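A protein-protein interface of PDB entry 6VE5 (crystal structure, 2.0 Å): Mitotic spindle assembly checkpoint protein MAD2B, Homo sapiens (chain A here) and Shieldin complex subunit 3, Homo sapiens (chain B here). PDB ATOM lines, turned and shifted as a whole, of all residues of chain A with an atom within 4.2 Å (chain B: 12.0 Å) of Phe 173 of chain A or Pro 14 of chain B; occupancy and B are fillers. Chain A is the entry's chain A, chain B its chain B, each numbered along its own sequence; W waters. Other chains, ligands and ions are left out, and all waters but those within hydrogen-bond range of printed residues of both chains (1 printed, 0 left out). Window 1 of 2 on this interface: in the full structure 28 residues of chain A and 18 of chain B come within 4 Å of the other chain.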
ATOM      1  N   TYR A  67      19.985  19.322  15.186  1.00  0.00           N
ATOM      2  CA  TYR A  67      18.976  19.585  16.209  1.00  0.00           C
ATOM      3  C   TYR A  67      19.301  18.847  17.496  1.00  0.00           C
ATOM      4  O   TYR A  67      19.239  19.420  18.588  1.00  0.00           O
ATOM      5  CB  TYR A  67      17.593  19.185  15.696  1.00  0.00           C
ATOM      6  CG  TYR A  67      16.481  19.449  16.683  1.00  0.00           C
ATOM      7  CD1 TYR A  67      15.725  20.614  16.609  1.00  0.00           C
ATOM      8  CD2 TYR A  67      16.184  18.534  17.687  1.00  0.00           C
ATOM      9  CE1 TYR A  67      14.696  20.859  17.515  1.00  0.00           C
ATOM     10  CE2 TYR A  67      15.160  18.768  18.591  1.00  0.00           C
ATOM     11  CZ  TYR A  67      14.423  19.934  18.496  1.00  0.00           C
ATOM     12  OH  TYR A  67      13.416  20.173  19.390  1.00  0.00           O
ATOM     13  N   ASP A  70      22.494  20.423  18.978  1.00  0.00           N
ATOM     14  CA  ASP A  70      22.178  21.718  19.574  1.00  0.00           C
ATOM     15  C   ASP A  70      21.488  21.541  20.925  1.00  0.00           C
ATOM     16  O   ASP A  70      21.810  22.240  21.894  1.00  0.00           O
ATOM     17  CB  ASP A  70      21.296  22.542  18.635  1.00  0.00           C
ATOM     18  CG  ASP A  70      22.076  23.149  17.474  1.00  0.00           C
ATOM     19  OD1 ASP A  70      23.322  23.124  17.493  1.00  0.00           O
ATOM     20  OD2 ASP A  70      21.435  23.646  16.530  1.00  0.00           O
ATOM     21  N   THR A  71      20.550  20.597  21.011  1.00  0.00           N
ATOM     22  CA  THR A  71      19.849  20.352  22.266  1.00  0.00           C
ATOM     23  C   THR A  71      20.827  19.988  23.378  1.00  0.00           C
ATOM     24  O   THR A  71      20.744  20.512  24.494  1.00  0.00           O
ATOM     25  CB  THR A  71      18.817  19.232  22.081  1.00  0.00           C
ATOM     26  OG1 THR A  71      17.853  19.615  21.088  1.00  0.00           O
ATOM     27  CG2 THR A  71      18.101  18.934  23.387  1.00  0.00           C
ATOM     28  N   CYS A  74      23.236  22.652  24.784  1.00  0.00           N
ATOM     29  CA  CYS A  74      22.594  23.496  25.788  1.00  0.00           C
ATOM     30  C   CYS A  74      22.538  22.814  27.151  1.00  0.00           C
ATOM     31  O   CYS A  74      22.610  23.489  28.180  1.00  0.00           O
ATOM     32  CB  CYS A  74      21.185  23.867  25.326  1.00  0.00           C
ATOM     33  SG  CYS A  74      21.134  24.961  23.867  1.00  0.00           S
ATOM     34  N   VAL A 152      12.624  16.917  23.721  1.00  0.00           N
ATOM     35  CA  VAL A 152      13.495  16.631  24.855  1.00  0.00           C
ATOM     36  C   VAL A 152      13.133  17.567  25.998  1.00  0.00           C
ATOM     37  O   VAL A 152      13.062  18.785  25.810  1.00  0.00           O
ATOM     38  CB  VAL A 152      14.982  16.770  24.482  1.00  0.00           C
ATOM     39  CG1 VAL A 152      15.852  16.598  25.709  1.00  0.00           C
ATOM     40  CG2 VAL A 152      15.354  15.759  23.406  1.00  0.00           C
ATOM     41  N   GLN A 168      20.586  28.648  27.517  1.00  0.00           N
ATOM     42  CA  GLN A 168      20.553  29.281  26.196  1.00  0.00           C
ATOM     43  C   GLN A 168      21.973  29.407  25.644  1.00  0.00           C
ATOM     44  O   GLN A 168      22.508  30.500  25.446  1.00  0.00           O
ATOM     45  CB  GLN A 168      19.879  30.644  26.275  1.00  0.00           C
ATOM     46  CG  GLN A 168      18.568  30.657  27.027  1.00  0.00           C
ATOM     47  CD  GLN A 168      17.399  30.201  26.179  1.00  0.00           C
ATOM     48  OE1 GLN A 168      17.573  29.498  25.186  1.00  0.00           O
ATOM     49  NE2 GLN A 168      16.198  30.609  26.565  1.00  0.00           N
ATOM     50  N   ILE A 170      23.102  28.122  22.620  1.00  0.00           N
ATOM     51  CA  ILE A 170      23.212  28.164  21.166  1.00  0.00           C
ATOM     52  C   ILE A 170      22.379  29.315  20.626  1.00  0.00           C
ATOM     53  O   ILE A 170      21.206  29.473  20.992  1.00  0.00           O
ATOM     54  CB  ILE A 170      22.758  26.832  20.536  1.00  0.00           C
ATOM     55  CG1 ILE A 170      23.675  25.681  20.957  1.00  0.00           C
ATOM     56  CG2 ILE A 170      22.712  26.958  19.014  1.00  0.00           C
ATOM     57  CD1 ILE A 170      25.121  25.854  20.576  1.00  0.00           C
ATOM     58  N   LYS A 171      22.977  30.108  19.740  1.00  0.00           N
ATOM     59  CA  LYS A 171      22.244  31.164  19.056  1.00  0.00           C
ATOM     60  C   LYS A 171      21.121  30.571  18.214  1.00  0.00           C
ATOM     61  O   LYS A 171      21.301  29.566  17.526  1.00  0.00           O
ATOM     62  CB  LYS A 171      23.199  31.971  18.172  1.00  0.00           C
ATOM     63  CG  LYS A 171      22.517  32.943  17.207  1.00  0.00           C
ATOM     64  CD  LYS A 171      23.531  33.895  16.584  1.00  0.00           C
ATOM     65  CE  LYS A 171      22.913  34.739  15.477  1.00  0.00           C
ATOM     66  NZ  LYS A 171      22.724  33.965  14.215  1.00  0.00           N
ATOM     67  N   ASP A 172      19.952  31.199  18.281  1.00  0.00           N
ATOM     68  CA  ASP A 172      18.780  30.814  17.500  1.00  0.00           C
ATOM     69  C   ASP A 172      18.228  29.452  17.888  1.00  0.00           C
ATOM     70  O   ASP A 172      17.528  28.817  17.088  1.00  0.00           O
ATOM     71  CB  ASP A 172      19.082  30.839  15.996  1.00  0.00           C
ATOM     72  CG  ASP A 172      19.339  32.241  15.473  1.00  0.00           C
ATOM     73  OD1 ASP A 172      19.126  33.210  16.232  1.00  0.00           O
ATOM     74  OD2 ASP A 172      19.760  32.372  14.304  1.00  0.00           O
ATOM     75  N   PHE A 173      18.523  28.978  19.097  1.00  0.00           N
ATOM     76  CA  PHE A 173      17.969  27.729  19.617  1.00  0.00           C
ATOM     77  C   PHE A 173      17.451  27.987  21.029  1.00  0.00           C
ATOM     78  O   PHE A 173      18.013  27.503  22.018  1.00  0.00           O
ATOM     79  CB  PHE A 173      19.006  26.608  19.592  1.00  0.00           C
ATOM     80  CG  PHE A 173      18.406  25.232  19.638  1.00  0.00           C
ATOM     81  CD1 PHE A 173      17.915  24.639  18.490  1.00  0.00           C
ATOM     82  CD2 PHE A 173      18.324  24.534  20.828  1.00  0.00           C
ATOM     83  CE1 PHE A 173      17.356  23.379  18.531  1.00  0.00           C
ATOM     84  CE2 PHE A 173      17.772  23.270  20.872  1.00  0.00           C
ATOM     85  CZ  PHE A 173      17.287  22.693  19.722  1.00  0.00           C
ATOM     86  N   PRO A 174      16.375  28.757  21.151  1.00  0.00           N
ATOM     87  CA  PRO A 174      15.870  29.110  22.483  1.00  0.00           C
ATOM     88  C   PRO A 174      15.146  27.958  23.158  1.00  0.00           C
ATOM     89  O   PRO A 174      14.597  27.060  22.511  1.00  0.00           O
ATOM     90  CB  PRO A 174      14.911  30.275  22.203  1.00  0.00           C
ATOM     91  CG  PRO A 174      14.468  30.059  20.791  1.00  0.00           C
ATOM     92  CD  PRO A 174      15.651  29.455  20.072  1.00  0.00           C
ATOM     93  N   TRP A 175      15.153  28.000  24.485  1.00  0.00           N
ATOM     94  CA  TRP A 175      14.415  27.070  25.323  1.00  0.00           C
ATOM     95  C   TRP A 175      13.266  27.806  26.002  1.00  0.00           C
ATOM     96  O   TRP A 175      13.333  29.017  26.224  1.00  0.00           O
ATOM     97  CB  TRP A 175      15.326  26.445  26.381  1.00  0.00           C
ATOM     98  CG  TRP A 175      16.328  25.481  25.824  1.00  0.00           C
ATOM     99  CD1 TRP A 175      17.396  25.779  25.033  1.00  0.00           C
ATOM    100  CD2 TRP A 175      16.362  24.062  26.028  1.00  0.00           C
ATOM    101  NE1 TRP A 175      18.097  24.635  24.731  1.00  0.00           N
ATOM    102  CE2 TRP A 175      17.481  23.567  25.331  1.00  0.00           C
ATOM    103  CE3 TRP A 175      15.553  23.164  26.732  1.00  0.00           C
ATOM    104  CZ2 TRP A 175      17.805  22.217  25.306  1.00  0.00           C
ATOM    105  CZ3 TRP A 175      15.877  21.824  26.714  1.00  0.00           C
ATOM    106  CH2 TRP A 175      16.997  21.360  26.011  1.00  0.00           C
ATOM    107  N   LEU B  10       7.949  22.252  36.467  1.00  0.00           N
ATOM    108  CA  LEU B  10       7.865  22.023  35.030  1.00  0.00           C
ATOM    109  C   LEU B  10       9.263  22.028  34.410  1.00  0.00           C
ATOM    110  O   LEU B  10      10.130  22.794  34.837  1.00  0.00           O
ATOM    111  CB  LEU B  10       7.002  23.093  34.366  1.00  0.00           C
ATOM    112  CG  LEU B  10       5.505  23.062  34.681  1.00  0.00           C
ATOM    113  CD1 LEU B  10       4.816  24.292  34.108  1.00  0.00           C
ATOM    114  CD2 LEU B  10       4.863  21.793  34.140  1.00  0.00           C
ATOM    115  N   PRO B  11       9.503  21.187  33.410  1.00  0.00           N
ATOM    116  CA  PRO B  11      10.824  21.148  32.772  1.00  0.00           C
ATOM    117  C   PRO B  11      10.955  22.204  31.685  1.00  0.00           C
ATOM    118  O   PRO B  11      10.003  22.891  31.313  1.00  0.00           O
ATOM    119  CB  PRO B  11      10.878  19.736  32.181  1.00  0.00           C
ATOM    120  CG  PRO B  11       9.449  19.455  31.810  1.00  0.00           C
ATOM    121  CD  PRO B  11       8.589  20.177  32.837  1.00  0.00           C
ATOM    122  N   LEU B  12      12.175  22.320  31.167  1.00  0.00           N
ATOM    123  CA  LEU B  12      12.448  23.149  30.006  1.00  0.00           C
ATOM    124  C   LEU B  12      12.435  22.277  28.755  1.00  0.00           C
ATOM    125  O   LEU B  12      12.692  21.071  28.816  1.00  0.00           O
ATOM    126  CB  LEU B  12      13.801  23.851  30.137  1.00  0.00           C
ATOM    127  CG  LEU B  12      14.009  24.656  31.419  1.00  0.00           C
ATOM    128  CD1 LEU B  12      15.296  25.459  31.359  1.00  0.00           C
ATOM    129  CD2 LEU B  12      12.820  25.565  31.671  1.00  0.00           C
ATOM    130  N   ARG B  13      12.134  22.893  27.617  1.00  0.00           N
ATOM    131  CA  ARG B  13      12.211  22.193  26.344  1.00  0.00           C
ATOM    132  C   ARG B  13      12.638  23.179  25.275  1.00  0.00           C
ATOM    133  O   ARG B  13      12.450  24.394  25.431  1.00  0.00           O
ATOM    134  CB  ARG B  13      10.875  21.540  25.968  1.00  0.00           C
ATOM    135  CG  ARG B  13       9.746  22.503  25.653  1.00  0.00           C
ATOM    136  CD  ARG B  13       8.582  21.753  25.008  1.00  0.00           C
ATOM    137  NE  ARG B  13       7.397  22.586  24.832  1.00  0.00           N
ATOM    138  CZ  ARG B  13       7.173  23.362  23.776  1.00  0.00           C
ATOM    139  NH1 ARG B  13       8.057  23.425  22.789  1.00  0.00           N
ATOM    140  NH2 ARG B  13       6.062  24.079  23.710  1.00  0.00           N
ATOM    141  N   PRO B  14      13.223  22.696  24.179  1.00  0.00           N
ATOM    142  CA  PRO B  14      13.538  23.600  23.066  1.00  0.00           C
ATOM    143  C   PRO B  14      12.271  24.191  22.481  1.00  0.00           C
ATOM    144  O   PRO B  14      11.236  23.524  22.389  1.00  0.00           O
ATOM    145  CB  PRO B  14      14.259  22.695  22.055  1.00  0.00           C
ATOM    146  CG  PRO B  14      14.709  21.502  22.851  1.00  0.00           C
ATOM    147  CD  PRO B  14      13.672  21.318  23.915  1.00  0.00           C
ATOM    148  N   LYS B  15      12.351  25.471  22.104  1.00  0.00           N
ATOM    149  CA  LYS B  15      11.229  26.102  21.427  1.00  0.00           C
ATOM    150  C   LYS B  15      11.049  25.529  20.028  1.00  0.00           C
ATOM    151  O   LYS B  15       9.916  25.351  19.564  1.00  0.00           O
ATOM    152  CB  LYS B  15      11.451  27.616  21.369  1.00  0.00           C
ATOM    153  CG  LYS B  15      10.244  28.408  20.904  1.00  0.00           C
ATOM    154  CD  LYS B  15      10.547  29.902  20.907  1.00  0.00           C
ATOM    155  CE  LYS B  15       9.370  30.716  20.394  1.00  0.00           C
ATOM    156  NZ  LYS B  15       9.792  32.072  19.939  1.00  0.00           N
ATOM    157  N   ARG B  16      12.148  25.245  19.340  1.00  0.00           N
ATOM    158  CA  ARG B  16      12.099  24.719  17.987  1.00  0.00           C
ATOM    159  C   ARG B  16      11.738  23.239  17.999  1.00  0.00           C
ATOM    160  O   ARG B  16      12.102  22.495  18.910  1.00  0.00           O
ATOM    161  CB  ARG B  16      13.445  24.902  17.283  1.00  0.00           C
ATOM    162  CG  ARG B  16      13.993  26.328  17.281  1.00  0.00           C
ATOM    163  CD  ARG B  16      13.600  27.085  16.025  1.00  0.00           C
ATOM    164  NE  ARG B  16      14.250  28.394  15.959  1.00  0.00           N
ATOM    165  CZ  ARG B  16      13.799  29.489  16.567  1.00  0.00           C
ATOM    166  NH1 ARG B  16      12.689  29.447  17.295  1.00  0.00           N
ATOM    167  NH2 ARG B  16      14.461  30.633  16.447  1.00  0.00           N
ATOM    168  N   SER B  17      11.038  22.823  16.986  1.00  0.00           N
ATOM    169  CA  SER B  17      10.689  21.426  16.814  1.00  0.00           C
ATOM    170  C   SER B  17      11.693  20.736  15.900  1.00  0.00           C
ATOM    171  O   SER B  17      12.307  21.380  15.041  1.00  0.00           O
ATOM    172  CB  SER B  17       9.287  21.293  16.217  1.00  0.00           C
ATOM    173  OG  SER B  17       8.345  22.027  16.979  1.00  0.00           O
ATOM    174  N   PRO B  18      11.900  19.432  16.064  1.00  0.00           N
ATOM    175  CA  PRO B  18      12.813  18.708  15.169  1.00  0.00           C
ATOM    176  C   PRO B  18      12.267  18.664  13.753  1.00  0.00           C
ATOM    177  O   PRO B  18      11.065  18.884  13.532  1.00  0.00           O
ATOM    178  CB  PRO B  18      12.880  17.305  15.787  1.00  0.00           C
ATOM    179  CG  PRO B  18      11.610  17.174  16.554  1.00  0.00           C
ATOM    180  CD  PRO B  18      11.306  18.548  17.077  1.00  0.00           C
ATOM    181  N   PRO B  19      13.117  18.361  12.772  1.00  0.00           N
ATOM    182  CA  PRO B  19      12.681  18.419  11.373  1.00  0.00           C
ATOM    183  C   PRO B  19      11.743  17.284  10.996  1.00  0.00           C
ATOM    184  O   PRO B  19      11.749  16.207  11.593  1.00  0.00           O
ATOM    185  CB  PRO B  19      13.998  18.323  10.593  1.00  0.00           C
ATOM    186  CG  PRO B  19      14.899  17.545  11.500  1.00  0.00           C
ATOM    187  CD  PRO B  19      14.531  17.957  12.899  1.00  0.00           C
HETATM  188  O   HOH W   1      15.034  25.702  20.275  1.00  0.00           O
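Among the printed residues, 15 pairs touch across the chains.
Tyr 67 of chain A touches four residues of chain B. No residue of chain B comes within 4 Å of Asp 70 of chain A. No residue of chain B comes within 4 Å of Thr 71 of chain A. Val 152 of chain A touches just these residues of chain B: Leu 12, Arg 13 and Pro 14. No residue of chain B comes within 4 Å of Gln 168 of chain A. Asp 172 of chain A touches one residue of chain B. Of the printed residues of chain B, Pro 174 of chain A touches Pro 14 (3.7 Å), Lys 15 (2.8 Å) and Arg 16 (3.96 Å). Trp 175 of chain A touches just these residues of chain B: Leu 12 (3.8 Å), Arg 13 (3.3 Å) and Pro 14 (3.5 Å). Of the printed residues of chain A, Leu 12 of chain B touches Val 152 and Trp 175. Of the printed residues of chain A, Arg 13 of chain B touches Val 152 (3.5 Å) and Trp 175 (3.3 Å). Of chain A, only Tyr 67, Val 152, Phe 173, Pro 174 and Trp 175 come within 4 Å of Pro 14 of chain B. Of the printed residues of chain A, Lys 15 of chain B touches Pro 174 (2.8 Å). Printed residues of chain A within 4 Å of Arg 16 of chain B: Tyr 67 (2.7 Å), Asp 172 (3.5 Å) and Pro 174 (3.96 Å). Printed residues of chain A within 4 Å of Ser 17 of chain B: Tyr 67 (3.4 Å). The nearest residue of chain B that does not touch Phe 173 of chain A is Arg 16 of chain B (4.4 Å). The nearest residue of chain A that does not touch Pro 14 of chain B is Thr 71 of chain A (4.1 Å).
The side-chain hydroxyl (OG1) of Thr 71 of chain A lies within hydrogen-bond range of the backbone carbonyl oxygen (O) of Tyr 67 of chain A (2.9 Å). The side-chain sulfur (SG) of Cys 74 of chain A sits at hydrogen-bond distance from the indole nitrogen (NE1) of Trp 175 of chain A, 3.2 Å away. The side-chain amide oxygen (OE1) of Gln 168 of chain A is in hydrogen-bond range of the backbone NH (N) of Trp 175 of chain A, at 2.9 Å. The side-chain amino group (NZ) of Lys 171 of chain A lies within salt-bridge range of the side-chain carboxylate (OD2) of Asp 172 of chain A (3.4 Å).
OH of Tyr 67 of chain A is in hydrogen-bond range of O of Arg 16 of chain B (2.7 Å). The backbone carbonyl oxygen of Asp 172 of chain A sits at hydrogen-bond distance from the guanidinium group of Arg 16 of chain B (3.5 Å). N of Lys 15 of chain B lies within hydrogen-bond range of O of Pro 174 of chain A (2.8 Å).
Among the printed residues, merely in contact across the chains: Val 152 of chain A with Pro 14 of chain B (3.2 Å), Trp 175 of chain A with Arg 13 of chain B (3.3 Å), Tyr 67 of chain A with Ser 17 of chain B (3.4 Å), Tyr 67 of chain A with Pro 18 of chain B (3.5 Å), Trp 175 of chain A with Pro 14 of chain B (3.5 Å), Val 152 of chain A with Arg 13 of chain B (3.5 Å), Pro 174 of chain A with Pro 14 of chain B (3.7 Å), Phe 173 of chain A with Pro 14 of chain B (3.8 Å), Tyr 67 of chain A with Pro 14 of chain B (3.8 Å), Val 152 of chain A with Leu 12 of chain B (3.8 Å), Trp 175 of chain A with Leu 12 of chain B (3.8 Å) and Pro 174 of chain A with Arg 16 of chain B (3.96 Å).
Water W1 lies within hydrogen-bond range of O of Pro 174 of chain A (2.7 Å), N of Arg 16 of chain B (3.1 Å) and N of Lys 15 of chain B (3.3 Å).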
